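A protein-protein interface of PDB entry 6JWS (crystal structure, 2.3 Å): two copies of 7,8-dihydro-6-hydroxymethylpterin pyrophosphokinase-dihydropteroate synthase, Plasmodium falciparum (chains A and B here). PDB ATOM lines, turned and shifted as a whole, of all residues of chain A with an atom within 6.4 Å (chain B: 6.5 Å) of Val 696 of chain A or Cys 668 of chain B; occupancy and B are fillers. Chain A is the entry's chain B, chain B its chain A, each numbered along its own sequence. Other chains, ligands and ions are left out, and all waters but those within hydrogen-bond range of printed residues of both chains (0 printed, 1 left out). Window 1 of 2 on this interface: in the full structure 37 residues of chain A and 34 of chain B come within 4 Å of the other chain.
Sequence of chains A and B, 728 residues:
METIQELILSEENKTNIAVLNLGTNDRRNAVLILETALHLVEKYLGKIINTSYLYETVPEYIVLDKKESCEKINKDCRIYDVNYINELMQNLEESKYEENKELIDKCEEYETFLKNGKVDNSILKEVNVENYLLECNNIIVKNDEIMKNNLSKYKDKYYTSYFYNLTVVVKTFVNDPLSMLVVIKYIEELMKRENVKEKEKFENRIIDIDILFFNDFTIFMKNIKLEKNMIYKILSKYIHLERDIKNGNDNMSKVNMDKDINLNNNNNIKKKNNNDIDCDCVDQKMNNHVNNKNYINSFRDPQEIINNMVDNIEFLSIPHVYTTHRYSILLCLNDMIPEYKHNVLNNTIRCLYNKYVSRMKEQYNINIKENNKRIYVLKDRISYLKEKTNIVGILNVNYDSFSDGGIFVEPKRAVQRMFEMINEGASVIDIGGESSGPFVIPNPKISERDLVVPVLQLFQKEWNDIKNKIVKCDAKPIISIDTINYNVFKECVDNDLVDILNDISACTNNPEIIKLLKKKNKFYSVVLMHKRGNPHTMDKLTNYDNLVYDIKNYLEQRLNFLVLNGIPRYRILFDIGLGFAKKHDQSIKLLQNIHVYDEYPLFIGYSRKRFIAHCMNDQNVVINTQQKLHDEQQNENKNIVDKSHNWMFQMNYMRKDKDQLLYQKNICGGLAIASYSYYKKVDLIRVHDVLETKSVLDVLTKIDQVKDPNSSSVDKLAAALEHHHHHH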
ATOM      1  N   MET A 648      -0.726  33.057 -31.651  1.00  0.00           N
ATOM      2  CA  MET A 648      -0.732  31.607 -31.711  1.00  0.00           C
ATOM      3  C   MET A 648      -1.322  31.128 -33.041  1.00  0.00           C
ATOM      4  O   MET A 648      -1.175  29.959 -33.395  1.00  0.00           O
ATOM      5  CB  MET A 648      -1.493  31.022 -30.516  1.00  0.00           C
ATOM      6  CG  MET A 648      -0.880  31.357 -29.157  1.00  0.00           C
ATOM      7  SD  MET A 648      -2.032  31.073 -27.772  1.00  0.00           S
ATOM      8  CE  MET A 648      -3.447  32.025 -28.314  1.00  0.00           C
ATOM      9  N   LEU A 671      -7.467  26.132 -25.301  1.00  0.00           N
ATOM     10  CA  LEU A 671      -6.544  25.668 -24.264  1.00  0.00           C
ATOM     11  C   LEU A 671      -7.281  25.520 -22.930  1.00  0.00           C
ATOM     12  O   LEU A 671      -6.926  24.676 -22.103  1.00  0.00           O
ATOM     13  CB  LEU A 671      -5.366  26.635 -24.122  1.00  0.00           C
ATOM     14  CG  LEU A 671      -4.434  26.775 -25.322  1.00  0.00           C
ATOM     15  CD1 LEU A 671      -3.430  27.912 -25.072  1.00  0.00           C
ATOM     16  CD2 LEU A 671      -3.712  25.471 -25.604  1.00  0.00           C
ATOM     17  N   ALA A 672      -8.317  26.338 -22.732  1.00  0.00           N
ATOM     18  CA  ALA A 672      -9.241  26.159 -21.620  1.00  0.00           C
ATOM     19  C   ALA A 672      -9.910  24.776 -21.702  1.00  0.00           C
ATOM     20  O   ALA A 672     -10.056  24.089 -20.688  1.00  0.00           O
ATOM     21  CB  ALA A 672     -10.263  27.283 -21.632  1.00  0.00           C
ATOM     22  N   ALA A 674      -8.679  22.206 -23.320  1.00  0.00           N
ATOM     23  CA  ALA A 674      -7.602  21.257 -23.043  1.00  0.00           C
ATOM     24  C   ALA A 674      -7.496  20.983 -21.540  1.00  0.00           C
ATOM     25  O   ALA A 674      -7.315  19.831 -21.139  1.00  0.00           O
ATOM     26  CB  ALA A 674      -6.280  21.744 -23.601  1.00  0.00           C
ATOM     27  N   SER A 675      -7.626  22.043 -20.723  1.00  0.00           N
ATOM     28  CA  SER A 675      -7.514  21.934 -19.266  1.00  0.00           C
ATOM     29  C   SER A 675      -8.662  21.108 -18.705  1.00  0.00           C
ATOM     30  O   SER A 675      -8.437  20.205 -17.902  1.00  0.00           O
ATOM     31  CB  SER A 675      -7.530  23.280 -18.591  1.00  0.00           C
ATOM     32  OG  SER A 675      -6.464  24.050 -19.089  1.00  0.00           O
ATOM     33  N   TYR A 678      -8.222  17.558 -19.640  1.00  0.00           N
ATOM     34  CA  TYR A 678      -7.225  16.976 -18.763  1.00  0.00           C
ATOM     35  C   TYR A 678      -7.869  16.544 -17.443  1.00  0.00           C
ATOM     36  O   TYR A 678      -7.645  15.421 -16.960  1.00  0.00           O
ATOM     37  CB  TYR A 678      -6.083  17.963 -18.505  1.00  0.00           C
ATOM     38  CG  TYR A 678      -5.142  17.436 -17.450  1.00  0.00           C
ATOM     39  CD1 TYR A 678      -4.117  16.563 -17.788  1.00  0.00           C
ATOM     40  CD2 TYR A 678      -5.337  17.739 -16.113  1.00  0.00           C
ATOM     41  CE1 TYR A 678      -3.277  16.038 -16.822  1.00  0.00           C
ATOM     42  CE2 TYR A 678      -4.515  17.217 -15.133  1.00  0.00           C
ATOM     43  CZ  TYR A 678      -3.481  16.369 -15.493  1.00  0.00           C
ATOM     44  OH  TYR A 678      -2.682  15.827 -14.532  1.00  0.00           O
ATOM     45  N   LEU A 691       1.977  22.728 -29.807  1.00  0.00           N
ATOM     46  CA  LEU A 691       2.940  23.251 -28.851  1.00  0.00           C
ATOM     47  C   LEU A 691       2.186  23.888 -27.690  1.00  0.00           C
ATOM     48  O   LEU A 691       2.552  23.709 -26.534  1.00  0.00           O
ATOM     49  CB  LEU A 691       3.855  24.278 -29.531  1.00  0.00           C
ATOM     50  CG  LEU A 691       4.783  25.033 -28.575  1.00  0.00           C
ATOM     51  CD1 LEU A 691       6.117  25.372 -29.253  1.00  0.00           C
ATOM     52  CD2 LEU A 691       4.102  26.300 -28.014  1.00  0.00           C
ATOM     53  N   GLU A 692       1.143  24.652 -28.015  1.00  0.00           N
ATOM     54  CA  GLU A 692       0.371  25.346 -27.000  1.00  0.00           C
ATOM     55  C   GLU A 692      -0.290  24.331 -26.058  1.00  0.00           C
ATOM     56  O   GLU A 692      -0.222  24.460 -24.842  1.00  0.00           O
ATOM     57  CB  GLU A 692      -0.662  26.235 -27.691  1.00  0.00           C
ATOM     58  CG  GLU A 692      -0.056  27.327 -28.565  1.00  0.00           C
ATOM     59  CD  GLU A 692       0.164  26.981 -30.034  1.00  0.00           C
ATOM     60  OE1 GLU A 692       0.707  25.892 -30.335  1.00  0.00           O
ATOM     61  OE2 GLU A 692      -0.233  27.803 -30.892  1.00  0.00           O
ATOM     62  N   THR A 693      -0.921  23.297 -26.633  1.00  0.00           N
ATOM     63  CA  THR A 693      -1.679  22.309 -25.880  1.00  0.00           C
ATOM     64  C   THR A 693      -0.740  21.505 -24.976  1.00  0.00           C
ATOM     65  O   THR A 693      -1.043  21.263 -23.805  1.00  0.00           O
ATOM     66  CB  THR A 693      -2.490  21.420 -26.840  1.00  0.00           C
ATOM     67  OG1 THR A 693      -3.313  22.285 -27.632  1.00  0.00           O
ATOM     68  CG2 THR A 693      -3.351  20.406 -26.120  1.00  0.00           C
ATOM     69  N   LYS A 694       0.400  21.078 -25.534  1.00  0.00           N
ATOM     70  CA  LYS A 694       1.389  20.325 -24.775  1.00  0.00           C
ATOM     71  C   LYS A 694       1.911  21.140 -23.587  1.00  0.00           C
ATOM     72  O   LYS A 694       2.214  20.567 -22.539  1.00  0.00           O
ATOM     73  CB  LYS A 694       2.558  19.933 -25.685  1.00  0.00           C
ATOM     74  CG  LYS A 694       3.561  18.949 -25.090  1.00  0.00           C
ATOM     75  CD  LYS A 694       2.926  17.628 -24.708  1.00  0.00           C
ATOM     76  CE  LYS A 694       3.921  16.514 -24.457  1.00  0.00           C
ATOM     77  NZ  LYS A 694       4.906  16.884 -23.415  1.00  0.00           N
ATOM     78  N   SER A 695       2.049  22.460 -23.762  1.00  0.00           N
ATOM     79  CA  SER A 695       2.578  23.300 -22.700  1.00  0.00           C
ATOM     80  C   SER A 695       1.597  23.285 -21.535  1.00  0.00           C
ATOM     81  O   SER A 695       2.017  23.194 -20.377  1.00  0.00           O
ATOM     82  CB  SER A 695       2.828  24.711 -23.171  1.00  0.00           C
ATOM     83  OG  SER A 695       3.761  24.719 -24.239  1.00  0.00           O
ATOM     84  N   VAL A 696       0.296  23.328 -21.872  1.00  0.00           N
ATOM     85  CA  VAL A 696      -0.767  23.301 -20.890  1.00  0.00           C
ATOM     86  C   VAL A 696      -0.772  21.958 -20.172  1.00  0.00           C
ATOM     87  O   VAL A 696      -0.798  21.906 -18.957  1.00  0.00           O
ATOM     88  CB  VAL A 696      -2.139  23.664 -21.501  1.00  0.00           C
ATOM     89  CG1 VAL A 696      -3.293  23.280 -20.572  1.00  0.00           C
ATOM     90  CG2 VAL A 696      -2.216  25.158 -21.823  1.00  0.00           C
ATOM     91  N   LEU A 697      -0.772  20.854 -20.916  1.00  0.00           N
ATOM     92  CA  LEU A 697      -0.858  19.551 -20.278  1.00  0.00           C
ATOM     93  C   LEU A 697       0.380  19.299 -19.405  1.00  0.00           C
ATOM     94  O   LEU A 697       0.286  18.629 -18.378  1.00  0.00           O
ATOM     95  CB  LEU A 697      -1.048  18.472 -21.356  1.00  0.00           C
ATOM     96  CG  LEU A 697      -2.315  18.578 -22.225  1.00  0.00           C
ATOM     97  CD1 LEU A 697      -2.366  17.442 -23.234  1.00  0.00           C
ATOM     98  CD2 LEU A 697      -3.595  18.569 -21.396  1.00  0.00           C
ATOM     99  N   ASP A 698       1.546  19.819 -19.816  1.00  0.00           N
ATOM    100  CA  ASP A 698       2.776  19.595 -19.061  1.00  0.00           C
ATOM    101  C   ASP A 698       2.683  20.220 -17.671  1.00  0.00           C
ATOM    102  O   ASP A 698       3.106  19.604 -16.706  1.00  0.00           O
ATOM    103  CB  ASP A 698       4.016  20.115 -19.790  1.00  0.00           C
ATOM    104  CG  ASP A 698       4.522  19.176 -20.885  1.00  0.00           C
ATOM    105  OD1 ASP A 698       4.006  18.033 -20.973  1.00  0.00           O
ATOM    106  OD2 ASP A 698       5.440  19.591 -21.651  1.00  0.00           O
ATOM    107  N   VAL A 699       2.128  21.435 -17.586  1.00  0.00           N
ATOM    108  CA  VAL A 699       2.009  22.167 -16.339  1.00  0.00           C
ATOM    109  C   VAL A 699       0.925  21.528 -15.472  1.00  0.00           C
ATOM    110  O   VAL A 699       1.110  21.421 -14.264  1.00  0.00           O
ATOM    111  CB  VAL A 699       1.681  23.647 -16.607  1.00  0.00           C
ATOM    112  CG1 VAL A 699       1.269  24.394 -15.341  1.00  0.00           C
ATOM    113  CG2 VAL A 699       2.812  24.354 -17.328  1.00  0.00           C
ATOM    114  N   LEU A 700      -0.211  21.126 -16.073  1.00  0.00           N
ATOM    115  CA  LEU A 700      -1.256  20.494 -15.272  1.00  0.00           C
ATOM    116  C   LEU A 700      -0.752  19.166 -14.694  1.00  0.00           C
ATOM    117  O   LEU A 700      -1.014  18.862 -13.531  1.00  0.00           O
ATOM    118  CB  LEU A 700      -2.562  20.360 -16.060  1.00  0.00           C
ATOM    119  CG  LEU A 700      -3.180  21.678 -16.559  1.00  0.00           C
ATOM    120  CD1 LEU A 700      -4.457  21.442 -17.347  1.00  0.00           C
ATOM    121  CD2 LEU A 700      -3.479  22.635 -15.409  1.00  0.00           C
ATOM    122  N   THR A 701       0.010  18.410 -15.496  1.00  0.00           N
ATOM    123  CA  THR A 701       0.598  17.151 -15.062  1.00  0.00           C
ATOM    124  C   THR A 701       1.559  17.373 -13.887  1.00  0.00           C
ATOM    125  O   THR A 701       1.576  16.576 -12.940  1.00  0.00           O
ATOM    126  CB  THR A 701       1.264  16.399 -16.231  1.00  0.00           C
ATOM    127  OG1 THR A 701       0.283  16.143 -17.247  1.00  0.00           O
ATOM    128  CG2 THR A 701       1.816  15.059 -15.799  1.00  0.00           C
ATOM    129  N   ILE B 612       7.554  27.959 -14.663  1.00  0.00           N
ATOM    130  CA  ILE B 612       6.690  27.408 -15.700  1.00  0.00           C
ATOM    131  C   ILE B 612       7.503  26.552 -16.680  1.00  0.00           C
ATOM    132  O   ILE B 612       7.131  25.397 -16.945  1.00  0.00           O
ATOM    133  CB  ILE B 612       5.895  28.520 -16.409  1.00  0.00           C
ATOM    134  CG1 ILE B 612       4.986  29.274 -15.428  1.00  0.00           C
ATOM    135  CG2 ILE B 612       5.116  27.941 -17.584  1.00  0.00           C
ATOM    136  CD1 ILE B 612       4.220  30.439 -16.051  1.00  0.00           C
ATOM    137  N   MET B 616       8.160  21.902 -18.189  1.00  0.00           N
ATOM    138  CA  MET B 616       8.032  21.419 -19.546  1.00  0.00           C
ATOM    139  C   MET B 616       9.085  20.392 -19.940  1.00  0.00           C
ATOM    140  O   MET B 616      10.228  20.422 -19.479  1.00  0.00           O
ATOM    141  CB  MET B 616       7.831  22.557 -20.543  1.00  0.00           C
ATOM    142  CG  MET B 616       6.347  22.881 -20.531  1.00  0.00           C
ATOM    143  SD  MET B 616       6.006  24.523 -20.969  1.00  0.00           S
ATOM    144  CE  MET B 616       4.672  24.916 -19.850  1.00  0.00           C
ATOM    145  N   TYR B 663       9.035  31.567 -25.184  1.00  0.00           N
ATOM    146  CA  TYR B 663       8.142  32.634 -24.776  1.00  0.00           C
ATOM    147  C   TYR B 663       6.689  32.158 -24.893  1.00  0.00           C
ATOM    148  O   TYR B 663       5.882  32.374 -23.986  1.00  0.00           O
ATOM    149  CB  TYR B 663       8.586  33.906 -25.512  1.00  0.00           C
ATOM    150  CG  TYR B 663       7.694  35.123 -25.505  1.00  0.00           C
ATOM    151  CD1 TYR B 663       7.685  36.025 -24.447  1.00  0.00           C
ATOM    152  CD2 TYR B 663       6.918  35.426 -26.612  1.00  0.00           C
ATOM    153  CE1 TYR B 663       6.888  37.163 -24.476  1.00  0.00           C
ATOM    154  CE2 TYR B 663       6.119  36.559 -26.659  1.00  0.00           C
ATOM    155  CZ  TYR B 663       6.100  37.427 -25.586  1.00  0.00           C
ATOM    156  OH  TYR B 663       5.295  38.527 -25.652  1.00  0.00           O
ATOM    157  N   GLN B 664       6.373  31.455 -25.984  1.00  0.00           N
ATOM    158  CA  GLN B 664       5.012  31.010 -26.220  1.00  0.00           C
ATOM    159  C   GLN B 664       4.657  29.899 -25.237  1.00  0.00           C
ATOM    160  O   GLN B 664       3.574  29.925 -24.658  1.00  0.00           O
ATOM    161  CB  GLN B 664       4.776  30.623 -27.684  1.00  0.00           C
ATOM    162  CG  GLN B 664       3.316  30.272 -27.962  1.00  0.00           C
ATOM    163  CD  GLN B 664       2.957  30.242 -29.427  1.00  0.00           C
ATOM    164  OE1 GLN B 664       2.165  31.051 -29.906  1.00  0.00           O
ATOM    165  NE2 GLN B 664       3.553  29.314 -30.156  1.00  0.00           N
ATOM    166  N   LYS B 665       5.581  28.951 -25.041  1.00  0.00           N
ATOM    167  CA  LYS B 665       5.382  27.859 -24.093  1.00  0.00           C
ATOM    168  C   LYS B 665       5.052  28.415 -22.706  1.00  0.00           C
ATOM    169  O   LYS B 665       4.144  27.939 -22.034  1.00  0.00           O
ATOM    170  CB  LYS B 665       6.633  26.988 -23.994  1.00  0.00           C
ATOM    171  CG  LYS B 665       6.926  26.121 -25.206  1.00  0.00           C
ATOM    172  CD  LYS B 665       7.893  25.022 -24.831  1.00  0.00           C
ATOM    173  CE  LYS B 665       8.329  24.178 -26.008  1.00  0.00           C
ATOM    174  NZ  LYS B 665       9.224  23.075 -25.577  1.00  0.00           N
ATOM    175  N   ASN B 666       5.792  29.451 -22.312  1.00  0.00           N
ATOM    176  CA  ASN B 666       5.621  30.145 -21.052  1.00  0.00           C
ATOM    177  C   ASN B 666       4.230  30.763 -20.970  1.00  0.00           C
ATOM    178  O   ASN B 666       3.533  30.600 -19.982  1.00  0.00           O
ATOM    179  CB  ASN B 666       6.647  31.264 -20.927  1.00  0.00           C
ATOM    180  CG  ASN B 666       7.636  31.018 -19.824  1.00  0.00           C
ATOM    181  OD1 ASN B 666       7.282  31.111 -18.652  1.00  0.00           O
ATOM    182  ND2 ASN B 666       8.879  30.756 -20.195  1.00  0.00           N
ATOM    183  N   ILE B 667       3.827  31.480 -22.014  1.00  0.00           N
ATOM    184  CA  ILE B 667       2.510  32.079 -21.966  1.00  0.00           C
ATOM    185  C   ILE B 667       1.472  30.963 -21.818  1.00  0.00           C
ATOM    186  O   ILE B 667       0.561  31.082 -20.990  1.00  0.00           O
ATOM    187  CB  ILE B 667       2.282  32.951 -23.211  1.00  0.00           C
ATOM    188  CG1 ILE B 667       3.190  34.182 -23.170  1.00  0.00           C
ATOM    189  CG2 ILE B 667       0.801  33.301 -23.386  1.00  0.00           C
ATOM    190  CD1 ILE B 667       3.172  34.997 -24.466  1.00  0.00           C
ATOM    191  N   CYS B 668       1.656  29.872 -22.586  1.00  0.00           N
ATOM    192  CA  CYS B 668       0.680  28.797 -22.603  1.00  0.00           C
ATOM    193  C   CYS B 668       0.680  28.045 -21.272  1.00  0.00           C
ATOM    194  O   CYS B 668      -0.393  27.706 -20.772  1.00  0.00           O
ATOM    195  CB  CYS B 668       0.847  27.886 -23.815  1.00  0.00           C
ATOM    196  SG  CYS B 668       0.518  28.764 -25.369  1.00  0.00           S
ATOM    197  N   GLY B 669       1.869  27.833 -20.689  1.00  0.00           N
ATOM    198  CA  GLY B 669       1.957  27.221 -19.374  1.00  0.00           C
ATOM    199  C   GLY B 669       1.240  28.062 -18.323  1.00  0.00           C
ATOM    200  O   GLY B 669       0.620  27.531 -17.406  1.00  0.00           O
ATOM    201  N   GLY B 670       1.305  29.390 -18.466  1.00  0.00           N
ATOM    202  CA  GLY B 670       0.587  30.253 -17.552  1.00  0.00           C
ATOM    203  C   GLY B 670      -0.927  30.085 -17.695  1.00  0.00           C
ATOM    204  O   GLY B 670      -1.653  30.173 -16.705  1.00  0.00           O
ATOM    205  N   LEU B 671      -1.399  29.827 -18.924  1.00  0.00           N
ATOM    206  CA  LEU B 671      -2.828  29.629 -19.163  1.00  0.00           C
ATOM    207  C   LEU B 671      -3.336  28.359 -18.481  1.00  0.00           C
ATOM    208  O   LEU B 671      -4.485  28.317 -18.046  1.00  0.00           O
ATOM    209  CB  LEU B 671      -3.142  29.677 -20.664  1.00  0.00           C
ATOM    210  CG  LEU B 671      -2.865  31.031 -21.329  1.00  0.00           C
ATOM    211  CD1 LEU B 671      -3.089  30.962 -22.842  1.00  0.00           C
ATOM    212  CD2 LEU B 671      -3.701  32.149 -20.706  1.00  0.00           C
ATOM    213  N   ALA B 672      -2.465  27.355 -18.322  1.00  0.00           N
ATOM    214  CA  ALA B 672      -2.756  26.182 -17.502  1.00  0.00           C
ATOM    215  C   ALA B 672      -2.933  26.581 -16.038  1.00  0.00           C
ATOM    216  O   ALA B 672      -3.858  26.108 -15.355  1.00  0.00           O
ATOM    217  CB  ALA B 672      -1.661  25.144 -17.637  1.00  0.00           C
ATOM    218  N   ILE B 673      -2.069  27.483 -15.553  1.00  0.00           N
ATOM    219  CA  ILE B 673      -2.197  27.916 -14.167  1.00  0.00           C
ATOM    220  C   ILE B 673      -3.448  28.777 -14.026  1.00  0.00           C
ATOM    221  O   ILE B 673      -4.121  28.693 -13.002  1.00  0.00           O
ATOM    222  CB  ILE B 673      -0.914  28.583 -13.608  1.00  0.00           C
ATOM    223  CG1 ILE B 673       0.285  27.645 -13.789  1.00  0.00           C
ATOM    224  CG2 ILE B 673      -1.130  28.954 -12.131  1.00  0.00           C
ATOM    225  CD1 ILE B 673       1.647  28.239 -13.465  1.00  0.00           C
ATOM    226  N   SER B 675      -6.205  28.177 -15.537  1.00  0.00           N
ATOM    227  CA  SER B 675      -7.262  27.166 -15.461  1.00  0.00           C
ATOM    228  C   SER B 675      -7.316  26.594 -14.051  1.00  0.00           C
ATOM    229  O   SER B 675      -8.390  26.499 -13.449  1.00  0.00           O
ATOM    230  CB  SER B 675      -7.044  26.036 -16.443  1.00  0.00           C
ATOM    231  OG  SER B 675      -7.153  26.542 -17.767  1.00  0.00           O
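OG of Ser 675 of chain A is in hydrogen-bond range of OG of Ser 675 of chain B (2.9 Å).
O of Leu 691 of chain A lies within hydrogen-bond range of OG of Ser 695 of chain A (2.8 Å).
The backbone carbonyl oxygen (O) of Gln 664 of chain B is in hydrogen-bond range of the side-chain sulfur (SG) of Cys 668 of chain B.
The backbone carbonyl oxygen (O) of Leu 671 of chain B sits at hydrogen-bond distance from the side-chain hydroxyl (OG) of Ser 675 of chain B.
O of Leu 671 of chain A lies within hydrogen-bond range of OG of Ser 675 of chain A (3.1 Å).
The side-chain amino group (NZ) of Lys 694 of chain A is in salt-bridge range of the side-chain carboxylate (OD1) of Asp 698 of chain A (2.8 Å).
Gln 664 of chain B touches Met 648 of chain A (OE1 to CG, 3.2 Å).
Leu 671 of chain A touches Leu 671 of chain B (CD1 to CD1, 3.8 Å).
Leu 691 of chain A touches Gln 664 of chain B (CD2 to NE2, 3.7 Å).
Glu 692 of chain A touches Cys 668 of chain B (CG to SG, 3.6 Å).
Ser 695 of chain A touches Met 616 of chain B.
Ser 695 of chain A touches Lys 665 of chain B (OG to CA, 3.5 Å).
Cys 668 of chain B touches Val 696 of chain A (O to CG2, 3.3 Å).
Val 699 of chain A touches Met 616 of chain B.
Val 699 of chain A touches Gly 669 of chain B.
Leu 700 of chain A touches Ala 672 of chain B.
Val 696 of chain A touches just these residues of chain B: Cys 668 (3.3 Å) and Ala 672 (3.6 Å).
Cys 668 of chain B touches three residues of chain A.
Of the printed residues of chain B, Asp 698 of chain A touches Met 616 (3.6 Å).
Of the printed residues of chain A, Leu 671 of chain B touches Leu 671 (3.8 Å).
Printed residues of chain B within 4 Å of Leu 671 of chain A: Leu 671.
Ala 674 of chain A touches none of the printed residues of chain B.
Leu 697 of chain A touches none of the printed residues of chain B.
The nearest residue of chain B that does not touch Val 696 of chain A is Leu 671 of chain B (4.8 Å).
The nearest residue of chain A that does not touch Cys 668 of chain B is Leu 671 of chain A (4.05 Å).
Of the 17 printed residues of chain A, 10 touch a printed residue of chain B.
Of the 14 printed residues of chain B, 9 touch a printed residue of chain A.
Among the printed residues, no Asp or Glu carboxylate lies within 4 Å of a Lys or Arg side-chain nitrogen of the other chain.
Leu 671 of chain A touches its own counterpart, Leu 671 of chain B.
Ser 675 of chain A touches its own counterpart, Ser 675 of chain B.
Of the 17 pairs that touch across the chains among the printed residues, 2 have their exchanged pair printed and touching as well.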
